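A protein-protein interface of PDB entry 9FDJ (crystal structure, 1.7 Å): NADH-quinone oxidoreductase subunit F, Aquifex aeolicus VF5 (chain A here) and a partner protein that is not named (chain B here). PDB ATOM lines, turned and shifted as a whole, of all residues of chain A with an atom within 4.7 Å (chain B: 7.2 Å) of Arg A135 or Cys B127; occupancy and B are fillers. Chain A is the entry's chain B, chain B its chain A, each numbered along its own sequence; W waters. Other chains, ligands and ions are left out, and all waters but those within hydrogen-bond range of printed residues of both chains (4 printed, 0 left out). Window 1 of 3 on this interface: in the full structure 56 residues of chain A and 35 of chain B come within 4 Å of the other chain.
NE2 of His B35 sits at hydrogen-bond distance from O of Gly A176 (2.8 Å). SG of Cys B127 lies close to N of Gly A99, 3.8 Å away. The guanidinium group (NH2) of Arg A135 is in hydrogen-bond range of the backbone carbonyl oxygen (O) of Cys B127 (2.8 Å). The side-chain sulfur (SG) of Cys B131 lies close to the backbone NH (N) of Gly A99, at 3.3 Å. The side-chain carboxylate (OE2) of Glu A137 sits close to the side-chain sulfur (SD) of Met B72.
The side-chain hydroxyl (OG) of Ser B88 lies within hydrogen-bond range of the backbone NH (N) of Cys B127 (2.8 Å). SG of Cys B127 lies close to N of Gly B129, at 3.4 Å. The backbone carbonyl oxygen of Ala A93 sits at hydrogen-bond distance from the backbone NH of Arg A135 (3.1 Å). The guanidinium group (NH1) of Arg A135 lies within hydrogen-bond range of the backbone carbonyl oxygen (O) of Glu A95. NE of Arg A135 lies close to OG of Ser A96. N of Gly A176 is in hydrogen-bond range of O of Ile A134, 2.8 Å away.
Among the printed residues, merely in contact across the chains: Glu A97 with Cys B127 (3.9 Å), Pro A98 with Ile B89 (3.9 Å), Pro A98 with Cys B127 (3.6 Å), Arg A135 with Leu B128 (3.5 Å), Arg A135 with Gly B129 (3.6 Å), Gly A136 with Met B72 (3.7 Å), Glu A137 with Leu B128 (3.8 Å), Tyr A138 with Leu B128 (3.5 Å) and Tyr A138 with Gly B129 (3.5 Å).
Arg A135 touches just these residues of chain B: Cys B127, Leu B128 and Gly B129. Cys B127 touches just these residues of chain A: Glu A97 (3.9 Å), Pro A98 (3.6 Å), Gly A99 (3.8 Å) and Arg A135 (2.8 Å). Printed residues of chain A within 4 Å of His B35: Gly A176. Printed residues of chain A within 4 Å of Met B72: Gly A136 and Glu A137. Of the printed residues of chain A, Ile B89 touches Pro A98 (3.9 Å). Of the printed residues of chain B, Gly A136 touches Met B72 (3.7 Å). Cys B91 touches none of the printed residues of chain A. Glu A95 touches none of the printed residues of chain B. The nearest residue of chain B that does not touch Arg A135 is Gln B126 (4.6 Å). The nearest residue of chain A that does not touch Cys B127 is Ser A96 (4.4 Å).
Hydrophobic or aromatic side chains of chain B that line the printed part of chain A: His B35, Met B72, Ile B89 and Leu B128. Printed residues of chain A that touch a printed residue of chain B: Glu A97, Pro A98, Gly A99, Arg A135, Gly A136, Glu A137, Tyr A138 and Gly A176. Among the printed residues, no Asp or Glu carboxylate lies within 4 Å of a Lys or Arg side-chain nitrogen of the other chain.
Water W3 lies within hydrogen-bond range of the backbone carbonyl oxygen (O) of Leu B128 (2.6 Å) and the backbone carbonyl oxygen (O) of Glu A137 (2.7 Å). Water W1 lies within hydrogen-bond range of O of Ser A96 (2.7 Å) and O of Cys B127 (2.8 Å). Water W2 lies within hydrogen-bond range of the backbone carbonyl oxygen of Gln B126 (2.8 Å), the guanidinium group of Arg A135 (3.1 Å) and the side-chain carboxylate of Glu A137 (3.4 Å). Water W4 lies within hydrogen-bond range of the guanidinium group of Arg A135 (3.2 Å), the backbone carbonyl oxygen of Glu A97 (3.2 Å), the backbone carbonyl oxygen of Glu A95 (3.3 Å) and the backbone NH of Gly B129 (3.4 Å).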
ATOM      1  N   ALA A  93      27.395 -19.698  23.793  1.00  0.00           N
ATOM      2  CA  ALA A  93      26.808 -19.459  22.489  1.00  0.00           C
ATOM      3  C   ALA A  93      26.889 -17.981  22.120  1.00  0.00           C
ATOM      4  O   ALA A  93      26.001 -17.440  21.453  1.00  0.00           O
ATOM      5  CB  ALA A  93      25.359 -19.926  22.512  1.00  0.00           C
ATOM      6  N   ASP A  94      27.976 -17.319  22.542  1.00  0.00           N
ATOM      7  CA  ASP A  94      28.130 -15.905  22.256  1.00  0.00           C
ATOM      8  C   ASP A  94      28.607 -15.621  20.833  1.00  0.00           C
ATOM      9  O   ASP A  94      28.448 -14.484  20.404  1.00  0.00           O
ATOM     10  CB  ASP A  94      29.037 -15.171  23.228  1.00  0.00           C
ATOM     11  CG  ASP A  94      28.754 -13.674  23.216  1.00  0.00           C
ATOM     12  OD1 ASP A  94      27.583 -13.327  23.497  1.00  0.00           O
ATOM     13  OD2 ASP A  94      29.654 -12.897  22.771  1.00  0.00           O
ATOM     14  N   GLU A  95      29.241 -16.613  20.182  1.00  0.00           N
ATOM     15  CA  GLU A  95      29.772 -16.559  18.820  1.00  0.00           C
ATOM     16  C   GLU A  95      29.638 -15.195  18.133  1.00  0.00           C
ATOM     17  O   GLU A  95      28.657 -14.923  17.431  1.00  0.00           O
ATOM     18  CB  GLU A  95      29.066 -17.628  17.994  1.00  0.00           C
ATOM     19  CG  GLU A  95      29.552 -17.683  16.554  1.00  0.00           C
ATOM     20  CD  GLU A  95      29.094 -18.925  15.839  1.00  0.00           C
ATOM     21  OE1 GLU A  95      27.875 -18.981  15.516  1.00  0.00           O
ATOM     22  OE2 GLU A  95      29.957 -19.804  15.619  1.00  0.00           O
ATOM     23  N   SER A  96      30.662 -14.352  18.294  1.00  0.00           N
ATOM     24  CA  SER A  96      30.634 -13.015  17.715  1.00  0.00           C
ATOM     25  C   SER A  96      31.946 -12.630  17.029  1.00  0.00           C
ATOM     26  O   SER A  96      32.117 -11.475  16.641  1.00  0.00           O
ATOM     27  CB  SER A  96      30.291 -12.005  18.803  1.00  0.00           C
ATOM     28  OG  SER A  96      28.939 -12.159  19.202  1.00  0.00           O
ATOM     29  N   GLU A  97      32.887 -13.563  16.904  1.00  0.00           N
ATOM     30  CA  GLU A  97      34.122 -13.258  16.202  1.00  0.00           C
ATOM     31  C   GLU A  97      33.842 -13.116  14.710  1.00  0.00           C
ATOM     32  O   GLU A  97      33.157 -13.957  14.137  1.00  0.00           O
ATOM     33  CB  GLU A  97      35.197 -14.323  16.368  1.00  0.00           C
ATOM     34  CG  GLU A  97      36.548 -13.777  15.892  1.00  0.00           C
ATOM     35  CD  GLU A  97      37.743 -14.619  16.237  1.00  0.00           C
ATOM     36  OE1 GLU A  97      37.617 -15.604  17.007  1.00  0.00           O
ATOM     37  OE2 GLU A  97      38.805 -14.258  15.714  1.00  0.00           O
ATOM     38  N   PRO A  98      34.372 -12.086  14.014  1.00  0.00           N
ATOM     39  CA  PRO A  98      34.207 -12.000  12.565  1.00  0.00           C
ATOM     40  C   PRO A  98      34.573 -13.292  11.848  1.00  0.00           C
ATOM     41  O   PRO A  98      35.595 -13.916  12.133  1.00  0.00           O
ATOM     42  CB  PRO A  98      35.124 -10.819  12.175  1.00  0.00           C
ATOM     43  CG  PRO A  98      35.054  -9.938  13.419  1.00  0.00           C
ATOM     44  CD  PRO A  98      35.158 -10.949  14.543  1.00  0.00           C
ATOM     45  N   GLY A  99      33.694 -13.691  10.921  1.00  0.00           N
ATOM     46  CA  GLY A  99      33.912 -14.864  10.105  1.00  0.00           C
ATOM     47  C   GLY A  99      33.270 -16.104  10.731  1.00  0.00           C
ATOM     48  O   GLY A  99      33.208 -17.138  10.089  1.00  0.00           O
ATOM     49  N   TYR A 133      24.312 -19.105  27.307  1.00  0.00           N
ATOM     50  CA  TYR A 133      24.438 -17.685  27.057  1.00  0.00           C
ATOM     51  C   TYR A 133      24.548 -17.504  25.544  1.00  0.00           C
ATOM     52  O   TYR A 133      25.578 -17.859  24.966  1.00  0.00           O
ATOM     53  CB  TYR A 133      25.688 -17.117  27.727  1.00  0.00           C
ATOM     54  CG  TYR A 133      25.749 -15.600  27.737  1.00  0.00           C
ATOM     55  CD1 TYR A 133      26.240 -14.893  26.645  1.00  0.00           C
ATOM     56  CD2 TYR A 133      25.290 -14.874  28.825  1.00  0.00           C
ATOM     57  CE1 TYR A 133      26.313 -13.512  26.656  1.00  0.00           C
ATOM     58  CE2 TYR A 133      25.342 -13.488  28.845  1.00  0.00           C
ATOM     59  CZ  TYR A 133      25.874 -12.803  27.767  1.00  0.00           C
ATOM     60  OH  TYR A 133      25.948 -11.421  27.781  1.00  0.00           O
ATOM     61  N   ILE A 134      23.468 -16.998  24.936  1.00  0.00           N
ATOM     62  CA  ILE A 134      23.430 -16.810  23.492  1.00  0.00           C
ATOM     63  C   ILE A 134      23.460 -15.315  23.190  1.00  0.00           C
ATOM     64  O   ILE A 134      22.752 -14.519  23.819  1.00  0.00           O
ATOM     65  CB  ILE A 134      22.235 -17.541  22.852  1.00  0.00           C
ATOM     66  CG1 ILE A 134      22.313 -17.476  21.319  1.00  0.00           C
ATOM     67  CG2 ILE A 134      20.883 -17.035  23.361  1.00  0.00           C
ATOM     68  CD1 ILE A 134      21.325 -18.383  20.608  1.00  0.00           C
ATOM     69  N   ARG A 135      24.254 -14.928  22.181  1.00  0.00           N
ATOM     70  CA  ARG A 135      24.367 -13.516  21.838  1.00  0.00           C
ATOM     71  C   ARG A 135      22.986 -12.967  21.502  1.00  0.00           C
ATOM     72  O   ARG A 135      22.114 -13.694  21.015  1.00  0.00           O
ATOM     73  CB  ARG A 135      25.336 -13.270  20.673  1.00  0.00           C
ATOM     74  CG  ARG A 135      24.862 -13.900  19.368  1.00  0.00           C
ATOM     75  CD  ARG A 135      25.897 -13.710  18.259  1.00  0.00           C
ATOM     76  NE  ARG A 135      26.014 -12.296  17.898  1.00  0.00           N
ATOM     77  CZ  ARG A 135      26.752 -11.821  16.893  1.00  0.00           C
ATOM     78  NH1 ARG A 135      27.463 -12.652  16.156  1.00  0.00           N
ATOM     79  NH2 ARG A 135      26.764 -10.518  16.658  1.00  0.00           N
ATOM     80  N   GLY A 136      22.807 -11.675  21.767  1.00  0.00           N
ATOM     81  CA  GLY A 136      21.540 -10.999  21.570  1.00  0.00           C
ATOM     82  C   GLY A 136      21.109 -10.947  20.104  1.00  0.00           C
ATOM     83  O   GLY A 136      19.910 -10.858  19.830  1.00  0.00           O
ATOM     84  N   GLU A 137      22.086 -10.971  19.190  1.00  0.00           N
ATOM     85  CA  GLU A 137      21.841 -10.868  17.753  1.00  0.00           C
ATOM     86  C   GLU A 137      21.470 -12.222  17.134  1.00  0.00           C
ATOM     87  O   GLU A 137      21.296 -12.303  15.916  1.00  0.00           O
ATOM     88  CB  GLU A 137      23.005 -10.249  16.977  1.00  0.00           C
ATOM     89  CG  GLU A 137      23.446  -8.884  17.500  1.00  0.00           C
ATOM     90  CD  GLU A 137      24.382  -8.936  18.709  1.00  0.00           C
ATOM     91  OE1 GLU A 137      24.687 -10.030  19.254  1.00  0.00           O
ATOM     92  OE2 GLU A 137      24.856  -7.829  19.054  1.00  0.00           O
ATOM     93  N   TYR A 138      21.272 -13.255  17.971  1.00  0.00           N
ATOM     94  CA  TYR A 138      20.740 -14.547  17.568  1.00  0.00           C
ATOM     95  C   TYR A 138      19.342 -14.746  18.180  1.00  0.00           C
ATOM     96  O   TYR A 138      19.101 -15.679  18.984  1.00  0.00           O
ATOM     97  CB  TYR A 138      21.663 -15.699  17.969  1.00  0.00           C
ATOM     98  CG  TYR A 138      22.965 -15.929  17.208  1.00  0.00           C
ATOM     99  CD1 TYR A 138      23.261 -15.269  16.010  1.00  0.00           C
ATOM    100  CD2 TYR A 138      23.882 -16.858  17.665  1.00  0.00           C
ATOM    101  CE1 TYR A 138      24.437 -15.521  15.322  1.00  0.00           C
ATOM    102  CE2 TYR A 138      25.055 -17.123  16.980  1.00  0.00           C
ATOM    103  CZ  TYR A 138      25.331 -16.459  15.797  1.00  0.00           C
ATOM    104  OH  TYR A 138      26.489 -16.752  15.129  1.00  0.00           O
ATOM    105  N   GLY A 176      22.739 -12.223  25.454  1.00  0.00           N
ATOM    106  CA  GLY A 176      23.615 -11.075  25.410  1.00  0.00           C
ATOM    107  C   GLY A 176      22.888  -9.861  24.857  1.00  0.00           C
ATOM    108  O   GLY A 176      21.687  -9.918  24.567  1.00  0.00           O
ATOM    109  N   HIS B  35      15.789  -5.931  26.904  1.00  0.00           N
ATOM    110  CA  HIS B  35      15.348  -6.298  25.571  1.00  0.00           C
ATOM    111  C   HIS B  35      13.839  -6.121  25.454  1.00  0.00           C
ATOM    112  O   HIS B  35      13.338  -5.605  24.463  1.00  0.00           O
ATOM    113  CB  HIS B  35      15.725  -7.742  25.248  1.00  0.00           C
ATOM    114  CG  HIS B  35      17.134  -7.923  24.823  1.00  0.00           C
ATOM    115  ND1 HIS B  35      17.632  -7.332  23.684  1.00  0.00           N
ATOM    116  CD2 HIS B  35      18.106  -8.714  25.300  1.00  0.00           C
ATOM    117  CE1 HIS B  35      18.889  -7.742  23.510  1.00  0.00           C
ATOM    118  NE2 HIS B  35      19.198  -8.581  24.483  1.00  0.00           N
ATOM    119  N   MET B  72      23.398  -3.106  21.985  1.00  0.00           N
ATOM    120  CA  MET B  72      22.112  -3.312  21.346  1.00  0.00           C
ATOM    121  C   MET B  72      21.070  -2.314  21.857  1.00  0.00           C
ATOM    122  O   MET B  72      20.098  -2.046  21.153  1.00  0.00           O
ATOM    123  CB  MET B  72      21.609  -4.741  21.543  1.00  0.00           C
ATOM    124  CG  MET B  72      22.272  -5.714  20.590  1.00  0.00           C
ATOM    125  SD  MET B  72      21.546  -7.354  20.776  1.00  0.00           S
ATOM    126  CE  MET B  72      20.008  -7.191  19.860  1.00  0.00           C
ATOM    127  N   VAL B  85      22.875  -3.235  10.074  1.00  0.00           N
ATOM    128  CA  VAL B  85      23.681  -3.546   8.904  1.00  0.00           C
ATOM    129  C   VAL B  85      25.082  -3.906   9.382  1.00  0.00           C
ATOM    130  O   VAL B  85      25.728  -3.108  10.054  1.00  0.00           O
ATOM    131  CB  VAL B  85      23.700  -2.352   7.938  1.00  0.00           C
ATOM    132  CG1 VAL B  85      24.700  -2.552   6.802  1.00  0.00           C
ATOM    133  CG2 VAL B  85      22.301  -2.033   7.410  1.00  0.00           C
ATOM    134  N   CYS B  86      25.557  -5.095   9.007  1.00  0.00           N
ATOM    135  CA  CYS B  86      26.895  -5.489   9.401  1.00  0.00           C
ATOM    136  C   CYS B  86      27.923  -4.676   8.621  1.00  0.00           C
ATOM    137  O   CYS B  86      27.855  -4.624   7.393  1.00  0.00           O
ATOM    138  CB  CYS B  86      27.089  -6.972   9.198  1.00  0.00           C
ATOM    139  SG  CYS B  86      28.772  -7.488   9.577  1.00  0.00           S
ATOM    140  N   VAL B  87      28.892  -4.092   9.331  1.00  0.00           N
ATOM    141  CA  VAL B  87      29.939  -3.282   8.719  1.00  0.00           C
ATOM    142  C   VAL B  87      31.311  -3.912   8.958  1.00  0.00           C
ATOM    143  O   VAL B  87      32.336  -3.270   8.762  1.00  0.00           O
ATOM    144  CB  VAL B  87      29.870  -1.824   9.224  1.00  0.00           C
ATOM    145  CG1 VAL B  87      28.531  -1.193   8.880  1.00  0.00           C
ATOM    146  CG2 VAL B  87      30.130  -1.692  10.724  1.00  0.00           C
ATOM    147  N   SER B  88      31.344  -5.173   9.377  1.00  0.00           N
ATOM    148  CA  SER B  88      32.596  -5.868   9.673  1.00  0.00           C
ATOM    149  C   SER B  88      33.195  -6.443   8.393  1.00  0.00           C
ATOM    150  O   SER B  88      32.621  -6.301   7.315  1.00  0.00           O
ATOM    151  CB  SER B  88      32.398  -6.947  10.712  1.00  0.00           C
ATOM    152  OG  SER B  88      32.107  -6.387  11.983  1.00  0.00           O
ATOM    153  N   ILE B  89      34.344  -7.095   8.534  1.00  0.00           N
ATOM    154  CA  ILE B  89      35.231  -7.389   7.423  1.00  0.00           C
ATOM    155  C   ILE B  89      34.562  -8.168   6.287  1.00  0.00           C
ATOM    156  O   ILE B  89      34.727  -7.799   5.122  1.00  0.00           O
ATOM    157  CB  ILE B  89      36.511  -8.094   7.883  1.00  0.00           C
ATOM    158  CG1 ILE B  89      37.387  -8.356   6.633  1.00  0.00           C
ATOM    159  CG2 ILE B  89      36.219  -9.362   8.694  1.00  0.00           C
ATOM    160  CD1 ILE B  89      38.802  -8.755   6.932  1.00  0.00           C
ATOM    161  N   VAL B  90      33.854  -9.264   6.579  1.00  0.00           N
ATOM    162  CA  VAL B  90      33.376 -10.087   5.467  1.00  0.00           C
ATOM    163  C   VAL B  90      32.275  -9.363   4.690  1.00  0.00           C
ATOM    164  O   VAL B  90      32.307  -9.293   3.454  1.00  0.00           O
ATOM    165  CB  VAL B  90      32.935 -11.498   5.897  1.00  0.00           C
ATOM    166  CG1 VAL B  90      32.667 -12.367   4.675  1.00  0.00           C
ATOM    167  CG2 VAL B  90      33.972 -12.139   6.797  1.00  0.00           C
ATOM    168  N   CYS B  91      31.347  -8.744   5.407  1.00  0.00           N
ATOM    169  CA  CYS B  91      30.280  -8.013   4.757  1.00  0.00           C
ATOM    170  C   CYS B  91      30.849  -6.839   3.975  1.00  0.00           C
ATOM    171  O   CYS B  91      30.379  -6.545   2.870  1.00  0.00           O
ATOM    172  CB  CYS B  91      29.215  -7.634   5.769  1.00  0.00           C
ATOM    173  SG  CYS B  91      28.305  -9.094   6.341  1.00  0.00           S
ATOM    174  N   VAL B 125      26.370  -2.369  12.780  1.00  0.00           N
ATOM    175  CA  VAL B 125      26.721  -3.360  13.780  1.00  0.00           C
ATOM    176  C   VAL B 125      27.962  -4.118  13.319  1.00  0.00           C
ATOM    177  O   VAL B 125      28.282  -4.185  12.130  1.00  0.00           O
ATOM    178  CB  VAL B 125      25.580  -4.335  14.128  1.00  0.00           C
ATOM    179  CG1 VAL B 125      24.378  -3.590  14.695  1.00  0.00           C
ATOM    180  CG2 VAL B 125      25.179  -5.189  12.924  1.00  0.00           C
ATOM    181  N   GLN B 126      28.635  -4.706  14.307  1.00  0.00           N
ATOM    182  CA  GLN B 126      29.715  -5.647  14.079  1.00  0.00           C
ATOM    183  C   GLN B 126      29.152  -6.989  13.608  1.00  0.00           C
ATOM    184  O   GLN B 126      27.951  -7.242  13.687  1.00  0.00           O
ATOM    185  CB  GLN B 126      30.465  -5.769  15.400  1.00  0.00           C
ATOM    186  CG  GLN B 126      31.007  -4.440  15.915  1.00  0.00           C
ATOM    187  CD  GLN B 126      31.914  -3.741  14.928  1.00  0.00           C
ATOM    188  OE1 GLN B 126      32.966  -4.262  14.536  1.00  0.00           O
ATOM    189  NE2 GLN B 126      31.518  -2.546  14.503  1.00  0.00           N
ATOM    190  N   CYS B 127      30.054  -7.874  13.186  1.00  0.00           N
ATOM    191  CA  CYS B 127      29.725  -9.162  12.596  1.00  0.00           C
ATOM    192  C   CYS B 127      28.521  -9.821  13.265  1.00  0.00           C
ATOM    193  O   CYS B 127      28.524 -10.063  14.486  1.00  0.00           O
ATOM    194  CB  CYS B 127      30.930 -10.082  12.667  1.00  0.00           C
ATOM    195  SG  CYS B 127      30.642 -11.762  12.029  1.00  0.00           S
ATOM    196  N   LEU B 128      27.529 -10.161  12.426  1.00  0.00           N
ATOM    197  CA  LEU B 128      26.274 -10.757  12.856  1.00  0.00           C
ATOM    198  C   LEU B 128      26.334 -12.283  12.854  1.00  0.00           C
ATOM    199  O   LEU B 128      25.318 -12.946  13.072  1.00  0.00           O
ATOM    200  CB  LEU B 128      25.154 -10.261  11.947  1.00  0.00           C
ATOM    201  CG  LEU B 128      24.680  -8.839  12.209  1.00  0.00           C
ATOM    202  CD1 LEU B 128      23.731  -8.346  11.106  1.00  0.00           C
ATOM    203  CD2 LEU B 128      24.029  -8.765  13.581  1.00  0.00           C
ATOM    204  N   GLY B 129      27.492 -12.862  12.572  1.00  0.00           N
ATOM    205  CA  GLY B 129      27.587 -14.317  12.606  1.00  0.00           C
ATOM    206  C   GLY B 129      26.790 -14.974  11.476  1.00  0.00           C
ATOM    207  O   GLY B 129      26.147 -15.988  11.701  1.00  0.00           O
ATOM    208  N   ALA B 130      26.830 -14.386  10.277  1.00  0.00           N
ATOM    209  CA  ALA B 130      26.201 -14.974   9.101  1.00  0.00           C
ATOM    210  C   ALA B 130      27.039 -14.677   7.850  1.00  0.00           C
ATOM    211  O   ALA B 130      26.512 -14.445   6.775  1.00  0.00           O
ATOM    212  CB  ALA B 130      24.775 -14.468   8.979  1.00  0.00           C
ATOM    213  N   CYS B 131      28.362 -14.759   8.008  1.00  0.00           N
ATOM    214  CA  CYS B 131      29.314 -14.151   7.096  1.00  0.00           C
ATOM    215  C   CYS B 131      29.263 -14.823   5.712  1.00  0.00           C
ATOM    216  O   CYS B 131      29.556 -14.219   4.682  1.00  0.00           O
ATOM    217  CB  CYS B 131      30.711 -14.209   7.709  1.00  0.00           C
ATOM    218  SG  CYS B 131      30.764 -13.799   9.476  1.00  0.00           S
HETATM  219  O   HOH W   1      30.485  -9.337  16.367  1.00  0.00           O
HETATM  220  O   HOH W   2      26.429  -7.477  16.027  1.00  0.00           O
HETATM  221  O   HOH W   3      22.743 -12.662  13.617  1.00  0.00           O
HETATM  222  O   HOH W   4      30.016 -13.763  14.627  1.00  0.00           O
